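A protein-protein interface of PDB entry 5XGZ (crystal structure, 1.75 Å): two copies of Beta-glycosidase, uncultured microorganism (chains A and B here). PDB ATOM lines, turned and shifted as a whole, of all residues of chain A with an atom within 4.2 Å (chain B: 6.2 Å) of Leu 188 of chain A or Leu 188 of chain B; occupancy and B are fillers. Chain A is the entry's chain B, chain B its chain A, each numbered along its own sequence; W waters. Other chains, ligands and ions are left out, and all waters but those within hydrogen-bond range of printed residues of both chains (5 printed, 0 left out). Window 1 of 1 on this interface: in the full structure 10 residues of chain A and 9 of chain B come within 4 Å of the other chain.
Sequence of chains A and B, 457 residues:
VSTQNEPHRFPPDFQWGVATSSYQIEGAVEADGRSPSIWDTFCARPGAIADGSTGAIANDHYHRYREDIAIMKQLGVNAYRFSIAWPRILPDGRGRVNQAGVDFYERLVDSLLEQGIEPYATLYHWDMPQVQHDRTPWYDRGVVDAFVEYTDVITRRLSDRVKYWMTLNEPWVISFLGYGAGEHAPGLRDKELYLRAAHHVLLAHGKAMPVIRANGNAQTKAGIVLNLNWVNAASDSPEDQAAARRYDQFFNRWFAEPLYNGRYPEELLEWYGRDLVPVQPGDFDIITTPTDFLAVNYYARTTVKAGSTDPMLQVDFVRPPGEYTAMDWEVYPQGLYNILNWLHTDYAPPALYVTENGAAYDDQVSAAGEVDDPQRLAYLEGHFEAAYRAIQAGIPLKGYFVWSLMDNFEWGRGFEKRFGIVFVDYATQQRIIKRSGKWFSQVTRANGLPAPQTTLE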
ATOM      1  N   ARG A  45     -19.956  -7.951 -19.269  1.00  0.00           N
ATOM      2  CA  ARG A  45     -20.532  -9.265 -19.288  1.00  0.00           C
ATOM      3  C   ARG A  45     -20.613  -9.761 -20.697  1.00  0.00           C
ATOM      4  O   ARG A  45     -21.189  -9.092 -21.576  1.00  0.00           O
ATOM      5  CB  ARG A  45     -21.949  -9.247 -18.680  1.00  0.00           C
ATOM      6  CG  ARG A  45     -22.649 -10.603 -18.715  1.00  0.00           C
ATOM      7  CD  ARG A  45     -24.145 -10.521 -18.303  1.00  0.00           C
ATOM      8  NE  ARG A  45     -24.240 -10.026 -16.957  1.00  0.00           N
ATOM      9  CZ  ARG A  45     -25.413  -9.865 -16.300  1.00  0.00           C
ATOM     10  NH1 ARG A  45     -26.591 -10.254 -16.915  1.00  0.00           N
ATOM     11  NH2 ARG A  45     -25.399  -9.346 -15.037  1.00  0.00           N
ATOM     12  N   TYR A 139     -34.761  -2.645  -6.601  1.00  0.00           N
ATOM     13  CA  TYR A 139     -35.705  -3.496  -5.852  1.00  0.00           C
ATOM     14  C   TYR A 139     -35.683  -3.271  -4.346  1.00  0.00           C
ATOM     15  O   TYR A 139     -36.500  -3.807  -3.658  1.00  0.00           O
ATOM     16  CB  TYR A 139     -35.536  -4.947  -6.190  1.00  0.00           C
ATOM     17  CG  TYR A 139     -34.145  -5.494  -6.005  1.00  0.00           C
ATOM     18  CD1 TYR A 139     -33.597  -5.686  -4.720  1.00  0.00           C
ATOM     19  CD2 TYR A 139     -33.396  -5.911  -7.099  1.00  0.00           C
ATOM     20  CE1 TYR A 139     -32.359  -6.253  -4.536  1.00  0.00           C
ATOM     21  CE2 TYR A 139     -32.167  -6.482  -6.904  1.00  0.00           C
ATOM     22  CZ  TYR A 139     -31.648  -6.649  -5.624  1.00  0.00           C
ATOM     23  OH  TYR A 139     -30.402  -7.220  -5.514  1.00  0.00           O
ATOM     24  N   GLY A 178     -33.926  -4.021 -16.887  1.00  0.00           N
ATOM     25  CA  GLY A 178     -32.881  -4.114 -15.883  1.00  0.00           C
ATOM     26  C   GLY A 178     -32.989  -5.309 -14.936  1.00  0.00           C
ATOM     27  O   GLY A 178     -31.983  -5.914 -14.560  1.00  0.00           O
ATOM     28  N   TYR A 179     -34.221  -5.609 -14.524  1.00  0.00           N
ATOM     29  CA  TYR A 179     -34.449  -6.597 -13.504  1.00  0.00           C
ATOM     30  C   TYR A 179     -35.381  -7.736 -13.907  1.00  0.00           C
ATOM     31  O   TYR A 179     -35.360  -8.778 -13.219  1.00  0.00           O
ATOM     32  CB  TYR A 179     -34.962  -5.962 -12.201  1.00  0.00           C
ATOM     33  CG  TYR A 179     -34.042  -4.928 -11.618  1.00  0.00           C
ATOM     34  CD1 TYR A 179     -34.017  -3.588 -12.110  1.00  0.00           C
ATOM     35  CD2 TYR A 179     -33.159  -5.273 -10.619  1.00  0.00           C
ATOM     36  CE1 TYR A 179     -33.162  -2.647 -11.579  1.00  0.00           C
ATOM     37  CE2 TYR A 179     -32.298  -4.325 -10.053  1.00  0.00           C
ATOM     38  CZ  TYR A 179     -32.311  -3.013 -10.517  1.00  0.00           C
ATOM     39  OH  TYR A 179     -31.491  -2.120  -9.939  1.00  0.00           O
ATOM     40  N   GLY A 180     -36.155  -7.553 -14.980  1.00  0.00           N
ATOM     41  CA  GLY A 180     -37.105  -8.498 -15.400  1.00  0.00           C
ATOM     42  C   GLY A 180     -36.632  -9.324 -16.595  1.00  0.00           C
ATOM     43  O   GLY A 180     -36.930 -10.452 -16.629  1.00  0.00           O
ATOM     44  N   ALA A 181     -35.993  -8.730 -17.600  1.00  0.00           N
ATOM     45  CA  ALA A 181     -35.604  -9.428 -18.818  1.00  0.00           C
ATOM     46  C   ALA A 181     -34.092  -9.652 -18.873  1.00  0.00           C
ATOM     47  O   ALA A 181     -33.649 -10.425 -19.712  1.00  0.00           O
ATOM     48  CB  ALA A 181     -35.970  -8.615 -20.011  1.00  0.00           C
ATOM     49  N   GLY A 182     -33.321  -9.003 -17.987  1.00  0.00           N
ATOM     50  CA  GLY A 182     -31.893  -9.182 -17.872  1.00  0.00           C
ATOM     51  C   GLY A 182     -31.136  -8.543 -19.040  1.00  0.00           C
ATOM     52  O   GLY A 182     -29.961  -8.763 -19.163  1.00  0.00           O
ATOM     53  N   PRO A 186     -28.844  -3.821 -14.119  1.00  0.00           N
ATOM     54  CA  PRO A 186     -27.730  -4.700 -13.721  1.00  0.00           C
ATOM     55  C   PRO A 186     -27.824  -6.087 -14.277  1.00  0.00           C
ATOM     56  O   PRO A 186     -27.016  -6.897 -13.946  1.00  0.00           O
ATOM     57  CB  PRO A 186     -27.854  -4.727 -12.186  1.00  0.00           C
ATOM     58  CG  PRO A 186     -29.351  -4.637 -11.968  1.00  0.00           C
ATOM     59  CD  PRO A 186     -29.874  -3.686 -13.073  1.00  0.00           C
ATOM     60  N   GLY A 187     -28.766  -6.374 -15.150  1.00  0.00           N
ATOM     61  CA  GLY A 187     -28.844  -7.658 -15.829  1.00  0.00           C
ATOM     62  C   GLY A 187     -29.486  -8.827 -15.070  1.00  0.00           C
ATOM     63  O   GLY A 187     -29.076  -9.970 -15.227  1.00  0.00           O
ATOM     64  N   LEU A 188     -30.513  -8.544 -14.283  1.00  0.00           N
ATOM     65  CA  LEU A 188     -31.290  -9.588 -13.578  1.00  0.00           C
ATOM     66  C   LEU A 188     -32.589  -9.918 -14.277  1.00  0.00           C
ATOM     67  O   LEU A 188     -33.117  -9.119 -15.015  1.00  0.00           O
ATOM     68  CB  LEU A 188     -31.568  -9.063 -12.167  1.00  0.00           C
ATOM     69  CG  LEU A 188     -30.491  -9.188 -11.088  1.00  0.00           C
ATOM     70  CD1 LEU A 188     -29.135  -9.487 -11.543  1.00  0.00           C
ATOM     71  CD2 LEU A 188     -30.518  -8.117 -10.029  1.00  0.00           C
ATOM     72  N   ARG A 189     -33.113 -11.097 -14.023  1.00  0.00           N
ATOM     73  CA  ARG A 189     -34.317 -11.590 -14.701  1.00  0.00           C
ATOM     74  C   ARG A 189     -35.295 -12.245 -13.717  1.00  0.00           C
ATOM     75  O   ARG A 189     -35.290 -13.487 -13.563  1.00  0.00           O
ATOM     76  CB  ARG A 189     -34.021 -12.626 -15.767  1.00  0.00           C
ATOM     77  CG  ARG A 189     -33.550 -12.111 -17.032  1.00  0.00           C
ATOM     78  CD  ARG A 189     -33.415 -13.212 -18.060  1.00  0.00           C
ATOM     79  NE  ARG A 189     -34.638 -13.830 -18.426  1.00  0.00           N
ATOM     80  CZ  ARG A 189     -34.734 -15.058 -18.946  1.00  0.00           C
ATOM     81  NH1 ARG A 189     -33.696 -15.853 -19.132  1.00  0.00           N
ATOM     82  NH2 ARG A 189     -35.927 -15.546 -19.210  1.00  0.00           N
ATOM     83  N   ASP A 190     -36.098 -11.454 -13.019  1.00  0.00           N
ATOM     84  CA  ASP A 190     -36.983 -11.994 -12.013  1.00  0.00           C
ATOM     85  C   ASP A 190     -38.254 -11.150 -11.983  1.00  0.00           C
ATOM     86  O   ASP A 190     -38.213  -9.925 -11.881  1.00  0.00           O
ATOM     87  CB  ASP A 190     -36.315 -12.033 -10.640  1.00  0.00           C
ATOM     88  CG  ASP A 190     -37.220 -12.630  -9.612  1.00  0.00           C
ATOM     89  OD1 ASP A 190     -37.549 -13.814  -9.850  1.00  0.00           O
ATOM     90  OD2 ASP A 190     -37.610 -11.955  -8.652  1.00  0.00           O
ATOM     91  N   PHE B  42     -25.914 -12.464  -1.863  1.00  0.00           N
ATOM     92  CA  PHE B  42     -27.144 -13.000  -2.464  1.00  0.00           C
ATOM     93  C   PHE B  42     -28.281 -13.130  -1.470  1.00  0.00           C
ATOM     94  O   PHE B  42     -29.456 -12.933  -1.865  1.00  0.00           O
ATOM     95  CB  PHE B  42     -26.833 -14.335  -3.134  1.00  0.00           C
ATOM     96  CG  PHE B  42     -27.982 -14.966  -3.827  1.00  0.00           C
ATOM     97  CD1 PHE B  42     -28.526 -14.353  -4.929  1.00  0.00           C
ATOM     98  CD2 PHE B  42     -28.540 -16.184  -3.389  1.00  0.00           C
ATOM     99  CE1 PHE B  42     -29.561 -14.945  -5.646  1.00  0.00           C
ATOM    100  CE2 PHE B  42     -29.609 -16.781  -4.093  1.00  0.00           C
ATOM    101  CZ  PHE B  42     -30.145 -16.142  -5.239  1.00  0.00           C
ATOM    102  N   ARG B  45     -30.860 -10.303  -1.202  1.00  0.00           N
ATOM    103  CA  ARG B  45     -31.855 -10.138  -2.234  1.00  0.00           C
ATOM    104  C   ARG B  45     -33.271 -10.614  -1.855  1.00  0.00           C
ATOM    105  O   ARG B  45     -33.573 -11.810  -1.536  1.00  0.00           O
ATOM    106  CB  ARG B  45     -31.416 -10.764  -3.581  1.00  0.00           C
ATOM    107  CG  ARG B  45     -32.444 -10.672  -4.713  1.00  0.00           C
ATOM    108  CD  ARG B  45     -32.192 -11.653  -5.899  1.00  0.00           C
ATOM    109  NE  ARG B  45     -30.950 -11.283  -6.513  1.00  0.00           N
ATOM    110  CZ  ARG B  45     -30.415 -11.851  -7.604  1.00  0.00           C
ATOM    111  NH1 ARG B  45     -31.088 -12.812  -8.252  1.00  0.00           N
ATOM    112  NH2 ARG B  45     -29.200 -11.381  -8.014  1.00  0.00           N
ATOM    113  N   HIS B 133     -15.351 -12.595  -7.405  1.00  0.00           N
ATOM    114  CA  HIS B 133     -16.437 -12.717  -8.409  1.00  0.00           C
ATOM    115  C   HIS B 133     -16.580 -11.391  -9.239  1.00  0.00           C
ATOM    116  O   HIS B 133     -16.901 -11.425 -10.414  1.00  0.00           O
ATOM    117  CB  HIS B 133     -17.796 -13.037  -7.744  1.00  0.00           C
ATOM    118  CG  HIS B 133     -18.846 -13.460  -8.718  1.00  0.00           C
ATOM    119  ND1 HIS B 133     -19.750 -12.587  -9.281  1.00  0.00           N
ATOM    120  CD2 HIS B 133     -19.090 -14.666  -9.273  1.00  0.00           C
ATOM    121  CE1 HIS B 133     -20.520 -13.257 -10.116  1.00  0.00           C
ATOM    122  NE2 HIS B 133     -20.136 -14.516 -10.138  1.00  0.00           N
ATOM    123  N   TYR B 139     -18.427 -17.356 -15.560  1.00  0.00           N
ATOM    124  CA  TYR B 139     -18.531 -17.178 -17.024  1.00  0.00           C
ATOM    125  C   TYR B 139     -17.339 -16.524 -17.637  1.00  0.00           C
ATOM    126  O   TYR B 139     -17.260 -16.452 -18.880  1.00  0.00           O
ATOM    127  CB  TYR B 139     -19.812 -16.494 -17.434  1.00  0.00           C
ATOM    128  CG  TYR B 139     -20.048 -15.130 -16.833  1.00  0.00           C
ATOM    129  CD1 TYR B 139     -19.260 -14.018 -17.193  1.00  0.00           C
ATOM    130  CD2 TYR B 139     -21.088 -14.918 -15.928  1.00  0.00           C
ATOM    131  CE1 TYR B 139     -19.482 -12.756 -16.667  1.00  0.00           C
ATOM    132  CE2 TYR B 139     -21.319 -13.645 -15.423  1.00  0.00           C
ATOM    133  CZ  TYR B 139     -20.541 -12.578 -15.809  1.00  0.00           C
ATOM    134  OH  TYR B 139     -20.813 -11.376 -15.233  1.00  0.00           O
ATOM    135  N   SER B 175     -23.129 -23.756 -12.069  1.00  0.00           N
ATOM    136  CA  SER B 175     -23.380 -23.086 -13.340  1.00  0.00           C
ATOM    137  C   SER B 175     -24.837 -22.835 -13.645  1.00  0.00           C
ATOM    138  O   SER B 175     -25.227 -21.710 -13.931  1.00  0.00           O
ATOM    139  CB  SER B 175     -22.777 -23.964 -14.473  1.00  0.00           C
ATOM    140  OG  SER B 175     -23.297 -25.241 -14.461  1.00  0.00           O
ATOM    141  N   PHE B 176     -25.658 -23.844 -13.619  1.00  0.00           N
ATOM    142  CA  PHE B 176     -27.079 -23.693 -13.923  1.00  0.00           C
ATOM    143  C   PHE B 176     -27.923 -22.917 -12.939  1.00  0.00           C
ATOM    144  O   PHE B 176     -28.658 -22.032 -13.348  1.00  0.00           O
ATOM    145  CB  PHE B 176     -27.781 -25.023 -14.312  1.00  0.00           C
ATOM    146  CG  PHE B 176     -29.203 -24.813 -14.686  1.00  0.00           C
ATOM    147  CD1 PHE B 176     -29.550 -24.144 -15.893  1.00  0.00           C
ATOM    148  CD2 PHE B 176     -30.232 -25.113 -13.794  1.00  0.00           C
ATOM    149  CE1 PHE B 176     -30.876 -23.870 -16.210  1.00  0.00           C
ATOM    150  CE2 PHE B 176     -31.596 -24.843 -14.136  1.00  0.00           C
ATOM    151  CZ  PHE B 176     -31.893 -24.210 -15.334  1.00  0.00           C
ATOM    152  N   LEU B 177     -27.843 -23.271 -11.655  1.00  0.00           N
ATOM    153  CA  LEU B 177     -28.601 -22.576 -10.622  1.00  0.00           C
ATOM    154  C   LEU B 177     -28.059 -21.194 -10.384  1.00  0.00           C
ATOM    155  O   LEU B 177     -28.798 -20.214 -10.153  1.00  0.00           O
ATOM    156  CB  LEU B 177     -28.704 -23.410  -9.323  1.00  0.00           C
ATOM    157  CG  LEU B 177     -29.580 -24.675  -9.370  1.00  0.00           C
ATOM    158  CD1 LEU B 177     -29.906 -25.227  -7.970  1.00  0.00           C
ATOM    159  CD2 LEU B 177     -30.903 -24.421 -10.089  1.00  0.00           C
ATOM    160  N   GLY B 178     -26.761 -21.075 -10.470  1.00  0.00           N
ATOM    161  CA  GLY B 178     -26.094 -19.762 -10.274  1.00  0.00           C
ATOM    162  C   GLY B 178     -26.227 -18.750 -11.431  1.00  0.00           C
ATOM    163  O   GLY B 178     -26.343 -17.573 -11.173  1.00  0.00           O
ATOM    164  N   TYR B 179     -26.167 -19.232 -12.668  1.00  0.00           N
ATOM    165  CA  TYR B 179     -26.141 -18.389 -13.833  1.00  0.00           C
ATOM    166  C   TYR B 179     -27.243 -18.653 -14.844  1.00  0.00           C
ATOM    167  O   TYR B 179     -27.502 -17.745 -15.658  1.00  0.00           O
ATOM    168  CB  TYR B 179     -24.760 -18.437 -14.534  1.00  0.00           C
ATOM    169  CG  TYR B 179     -23.608 -18.029 -13.691  1.00  0.00           C
ATOM    170  CD1 TYR B 179     -23.011 -18.957 -12.800  1.00  0.00           C
ATOM    171  CD2 TYR B 179     -23.152 -16.722 -13.684  1.00  0.00           C
ATOM    172  CE1 TYR B 179     -21.928 -18.602 -12.008  1.00  0.00           C
ATOM    173  CE2 TYR B 179     -22.060 -16.354 -12.889  1.00  0.00           C
ATOM    174  CZ  TYR B 179     -21.438 -17.300 -12.061  1.00  0.00           C
ATOM    175  OH  TYR B 179     -20.381 -16.951 -11.330  1.00  0.00           O
ATOM    176  N   GLY B 180     -27.887 -19.831 -14.772  1.00  0.00           N
ATOM    177  CA  GLY B 180     -28.894 -20.189 -15.692  1.00  0.00           C
ATOM    178  C   GLY B 180     -30.332 -20.039 -15.185  1.00  0.00           C
ATOM    179  O   GLY B 180     -31.183 -19.733 -15.938  1.00  0.00           O
ATOM    180  N   ALA B 181     -30.618 -20.354 -13.928  1.00  0.00           N
ATOM    181  CA  ALA B 181     -31.976 -20.303 -13.347  1.00  0.00           C
ATOM    182  C   ALA B 181     -32.114 -19.170 -12.355  1.00  0.00           C
ATOM    183  O   ALA B 181     -33.226 -18.839 -11.976  1.00  0.00           O
ATOM    184  CB  ALA B 181     -32.256 -21.581 -12.645  1.00  0.00           C
ATOM    185  N   GLY B 182     -31.009 -18.545 -11.937  1.00  0.00           N
ATOM    186  CA  GLY B 182     -31.059 -17.383 -11.025  1.00  0.00           C
ATOM    187  C   GLY B 182     -31.399 -17.787  -9.595  1.00  0.00           C
ATOM    188  O   GLY B 182     -31.660 -16.930  -8.780  1.00  0.00           O
ATOM    189  N   GLU B 183     -31.374 -19.068  -9.282  1.00  0.00           N
ATOM    190  CA  GLU B 183     -31.839 -19.550  -7.980  1.00  0.00           C
ATOM    191  C   GLU B 183     -30.762 -19.487  -6.910  1.00  0.00           C
ATOM    192  O   GLU B 183     -31.100 -19.434  -5.761  1.00  0.00           O
ATOM    193  CB  GLU B 183     -32.346 -20.990  -8.116  1.00  0.00           C
ATOM    194  CG  GLU B 183     -33.779 -21.018  -8.588  1.00  0.00           C
ATOM    195  CD  GLU B 183     -34.307 -22.434  -8.763  1.00  0.00           C
ATOM    196  OE1 GLU B 183     -33.906 -23.321  -7.975  1.00  0.00           O
ATOM    197  OE2 GLU B 183     -35.144 -22.592  -9.673  1.00  0.00           O
ATOM    198  N   HIS B 184     -29.489 -19.602  -7.311  1.00  0.00           N
ATOM    199  CA  HIS B 184     -28.317 -19.565  -6.430  1.00  0.00           C
ATOM    200  C   HIS B 184     -27.435 -18.377  -6.796  1.00  0.00           C
ATOM    201  O   HIS B 184     -27.520 -17.837  -7.908  1.00  0.00           O
ATOM    202  CB  HIS B 184     -27.470 -20.836  -6.586  1.00  0.00           C
ATOM    203  CG  HIS B 184     -28.010 -22.029  -5.854  1.00  0.00           C
ATOM    204  ND1 HIS B 184     -29.274 -22.084  -5.261  1.00  0.00           N
ATOM    205  CD2 HIS B 184     -27.448 -23.230  -5.649  1.00  0.00           C
ATOM    206  CE1 HIS B 184     -29.426 -23.263  -4.679  1.00  0.00           C
ATOM    207  NE2 HIS B 184     -28.348 -23.975  -4.941  1.00  0.00           N
ATOM    208  N   ALA B 185     -26.553 -17.976  -5.855  1.00  0.00           N
ATOM    209  CA  ALA B 185     -25.636 -16.896  -6.118  1.00  0.00           C
ATOM    210  C   ALA B 185     -24.789 -17.247  -7.349  1.00  0.00           C
ATOM    211  O   ALA B 185     -24.327 -18.378  -7.520  1.00  0.00           O
ATOM    212  CB  ALA B 185     -24.735 -16.687  -4.920  1.00  0.00           C
ATOM    213  N   PRO B 186     -24.533 -16.266  -8.201  1.00  0.00           N
ATOM    214  CA  PRO B 186     -24.811 -14.854  -8.035  1.00  0.00           C
ATOM    215  C   PRO B 186     -26.173 -14.440  -8.481  1.00  0.00           C
ATOM    216  O   PRO B 186     -26.460 -13.323  -8.365  1.00  0.00           O
ATOM    217  CB  PRO B 186     -23.743 -14.203  -8.901  1.00  0.00           C
ATOM    218  CG  PRO B 186     -23.550 -15.176 -10.029  1.00  0.00           C
ATOM    219  CD  PRO B 186     -23.629 -16.553  -9.339  1.00  0.00           C
ATOM    220  N   GLY B 187     -27.058 -15.361  -8.844  1.00  0.00           N
ATOM    221  CA  GLY B 187     -28.451 -15.063  -9.193  1.00  0.00           C
ATOM    222  C   GLY B 187     -28.715 -14.536 -10.602  1.00  0.00           C
ATOM    223  O   GLY B 187     -29.597 -13.691 -10.832  1.00  0.00           O
ATOM    224  N   LEU B 188     -27.982 -15.040 -11.569  1.00  0.00           N
ATOM    225  CA  LEU B 188     -28.219 -14.686 -13.003  1.00  0.00           C
ATOM    226  C   LEU B 188     -28.993 -15.768 -13.742  1.00  0.00           C
ATOM    227  O   LEU B 188     -29.009 -16.929 -13.351  1.00  0.00           O
ATOM    228  CB  LEU B 188     -26.865 -14.469 -13.606  1.00  0.00           C
ATOM    229  CG  LEU B 188     -26.128 -13.131 -13.482  1.00  0.00           C
ATOM    230  CD1 LEU B 188     -26.832 -12.033 -12.739  1.00  0.00           C
ATOM    231  CD2 LEU B 188     -24.653 -13.171 -13.273  1.00  0.00           C
ATOM    232  N   ARG B 189     -29.662 -15.381 -14.807  1.00  0.00           N
ATOM    233  CA  ARG B 189     -30.513 -16.290 -15.558  1.00  0.00           C
ATOM    234  C   ARG B 189     -30.284 -16.140 -17.068  1.00  0.00           C
ATOM    235  O   ARG B 189     -31.044 -15.451 -17.732  1.00  0.00           O
ATOM    236  CB  ARG B 189     -32.004 -16.096 -15.338  1.00  0.00           C
ATOM    237  CG  ARG B 189     -32.502 -16.582 -14.063  1.00  0.00           C
ATOM    238  CD  ARG B 189     -34.012 -16.418 -13.938  1.00  0.00           C
ATOM    239  NE  ARG B 189     -34.721 -17.046 -15.014  1.00  0.00           N
ATOM    240  CZ  ARG B 189     -35.977 -16.805 -15.343  1.00  0.00           C
ATOM    241  NH1 ARG B 189     -36.753 -15.964 -14.678  1.00  0.00           N
ATOM    242  NH2 ARG B 189     -36.475 -17.431 -16.384  1.00  0.00           N
ATOM    243  N   ASP B 190     -29.253 -16.775 -17.601  1.00  0.00           N
ATOM    244  CA  ASP B 190     -28.979 -16.670 -19.011  1.00  0.00           C
ATOM    245  C   ASP B 190     -28.362 -17.958 -19.502  1.00  0.00           C
ATOM    246  O   ASP B 190     -27.380 -18.468 -18.924  1.00  0.00           O
ATOM    247  CB  ASP B 190     -28.043 -15.454 -19.220  1.00  0.00           C
ATOM    248  CG  ASP B 190     -27.734 -15.260 -20.672  1.00  0.00           C
ATOM    249  OD1 ASP B 190     -28.740 -14.938 -21.415  1.00  0.00           O
ATOM    250  OD2 ASP B 190     -26.615 -15.544 -21.075  1.00  0.00           O
ATOM    251  N   LEU B 193     -24.518 -17.612 -20.267  1.00  0.00           N
ATOM    252  CA  LEU B 193     -23.697 -17.466 -19.061  1.00  0.00           C
ATOM    253  C   LEU B 193     -23.552 -18.801 -18.313  1.00  0.00           C
ATOM    254  O   LEU B 193     -22.457 -19.145 -17.829  1.00  0.00           O
ATOM    255  CB  LEU B 193     -24.315 -16.414 -18.174  1.00  0.00           C
ATOM    256  CG  LEU B 193     -23.810 -14.984 -18.246  1.00  0.00           C
ATOM    257  CD1 LEU B 193     -23.033 -14.530 -19.467  1.00  0.00           C
ATOM    258  CD2 LEU B 193     -24.872 -14.053 -17.731  1.00  0.00           C
HETATM  259  O   HOH W   1     -36.226 -15.422 -11.531  1.00  0.00           O
HETATM  260  O   HOH W   2     -37.460 -17.659 -18.754  1.00  0.00           O
HETATM  261  O   HOH W   3     -31.642 -13.104 -12.510  1.00  0.00           O
HETATM  262  O   HOH W   4     -30.025 -12.575 -15.515  1.00  0.00           O
HETATM  263  O   HOH W   5     -31.210 -14.319 -20.291  1.00  0.00           O
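O of Arg 189 of chain B sits at hydrogen-bond distance from NH1 of Arg 189 of chain A, 3.0 Å away.
The backbone carbonyl oxygen (O) of Gly 187 of chain A sits at hydrogen-bond distance from the guanidinium group (NH1) of Arg 45 of chain A (3.0 Å). The backbone carbonyl oxygen (O) of Gly 178 of chain A lies within hydrogen-bond range of the backbone NH (N) of Gly 187 of chain A (3.3 Å). The backbone NH of Leu 188 of chain A is in hydrogen-bond range of the backbone carbonyl oxygen of Gly 178 of chain A (3.0 Å). The guanidinium group (NH2) of Arg 45 of chain A lies within hydrogen-bond range of the backbone carbonyl oxygen (O) of Pro 186 of chain A, at 3.1 Å. O of Gly 178 of chain B lies within hydrogen-bond range of N of Leu 188 of chain B (3.0 Å). O of Leu 188 of chain A lies within hydrogen-bond range of N of Gly 182 of chain A (3.0 Å).
NH2 of Arg 45 of chain A touches CD1 of Leu 188 of chain B (3.8 Å). Arg 45 of chain A touches Leu 193 of chain B (CD to CD2, 3.7 Å). Gly 187 of chain A touches Leu 188 of chain B (O to CD1, 3.9 Å). Leu 188 of chain A touches Arg 45 of chain B. CD1 of Leu 188 of chain A touches CD1 of Leu 188 of chain B, 3.6 Å away.
Printed residues of chain B within 4 Å of Gly 187 of chain A: Leu 188 (3.9 Å). Printed residues of chain B within 4 Å of Leu 188 of chain A: Arg 45 and Leu 188. Of the printed residues of chain A, Arg 45 of chain B touches Leu 188. Of chain A, only Arg 45 (3.8 Å), Gly 187 (3.9 Å) and Leu 188 (3.6 Å) come within 4 Å of Leu 188 of chain B. Printed residues of chain A within 4 Å of Arg 189 of chain B: Arg 189 (3.0 Å).
Of the 21 printed residues of chain B, 4 touch a printed residue of chain A. Of the 12 printed residues of chain A, 4 touch a printed residue of chain B. Hydrophobic or aromatic side chains of chain A within 4 Å of the printed part of chain B: Leu 188. Among the printed residues, no Asp or Glu carboxylate lies within 4 Å of a Lys or Arg side-chain nitrogen of the other chain.
Arg 45 of chain A touches Leu 188 of chain B, and with the chains exchanged Leu 188 of chain A touches Arg 45 of chain B. Gly 187 of chain A touches Leu 188 of chain B, but with the chains exchanged Leu 188 of chain A does not touch Gly 187 of chain B (4.3 Å). Leu 188 of chain A touches its own counterpart, Leu 188 of chain B. Arg 189 of chain B touches its own counterpart, Arg 189 of chain A. Of the 6 pairs that touch across the chains among the printed residues, 4 have their exchanged pair printed and touching as well.
Water W2 bridges the guanidinium group (NH2) of Arg 189 of chain B (2.6 Å) and the guanidinium group (NH2) of Arg 189 of chain A (2.7 Å). Water W1 lies within hydrogen-bond range of OD1 of Asp 190 of chain A (2.7 Å), O of Arg 189 of chain A (3.0 Å) and NH1 of Arg 189 of chain B (3.2 Å). Water W3 bridges the backbone carbonyl oxygen (O) of Gly 187 of chain B (2.7 Å) and the backbone NH (N) of Arg 189 of chain A (2.9 Å). Water W5 lies within hydrogen-bond range of the side-chain carboxylate of Asp 190 of chain B (2.8 Å), the backbone carbonyl oxygen of Arg 189 of chain B (2.8 Å) and the guanidinium group of Arg 189 of chain A (3.1 Å). Water W4 bridges O of Gly 187 of chain A and N of Arg 189 of chain B.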
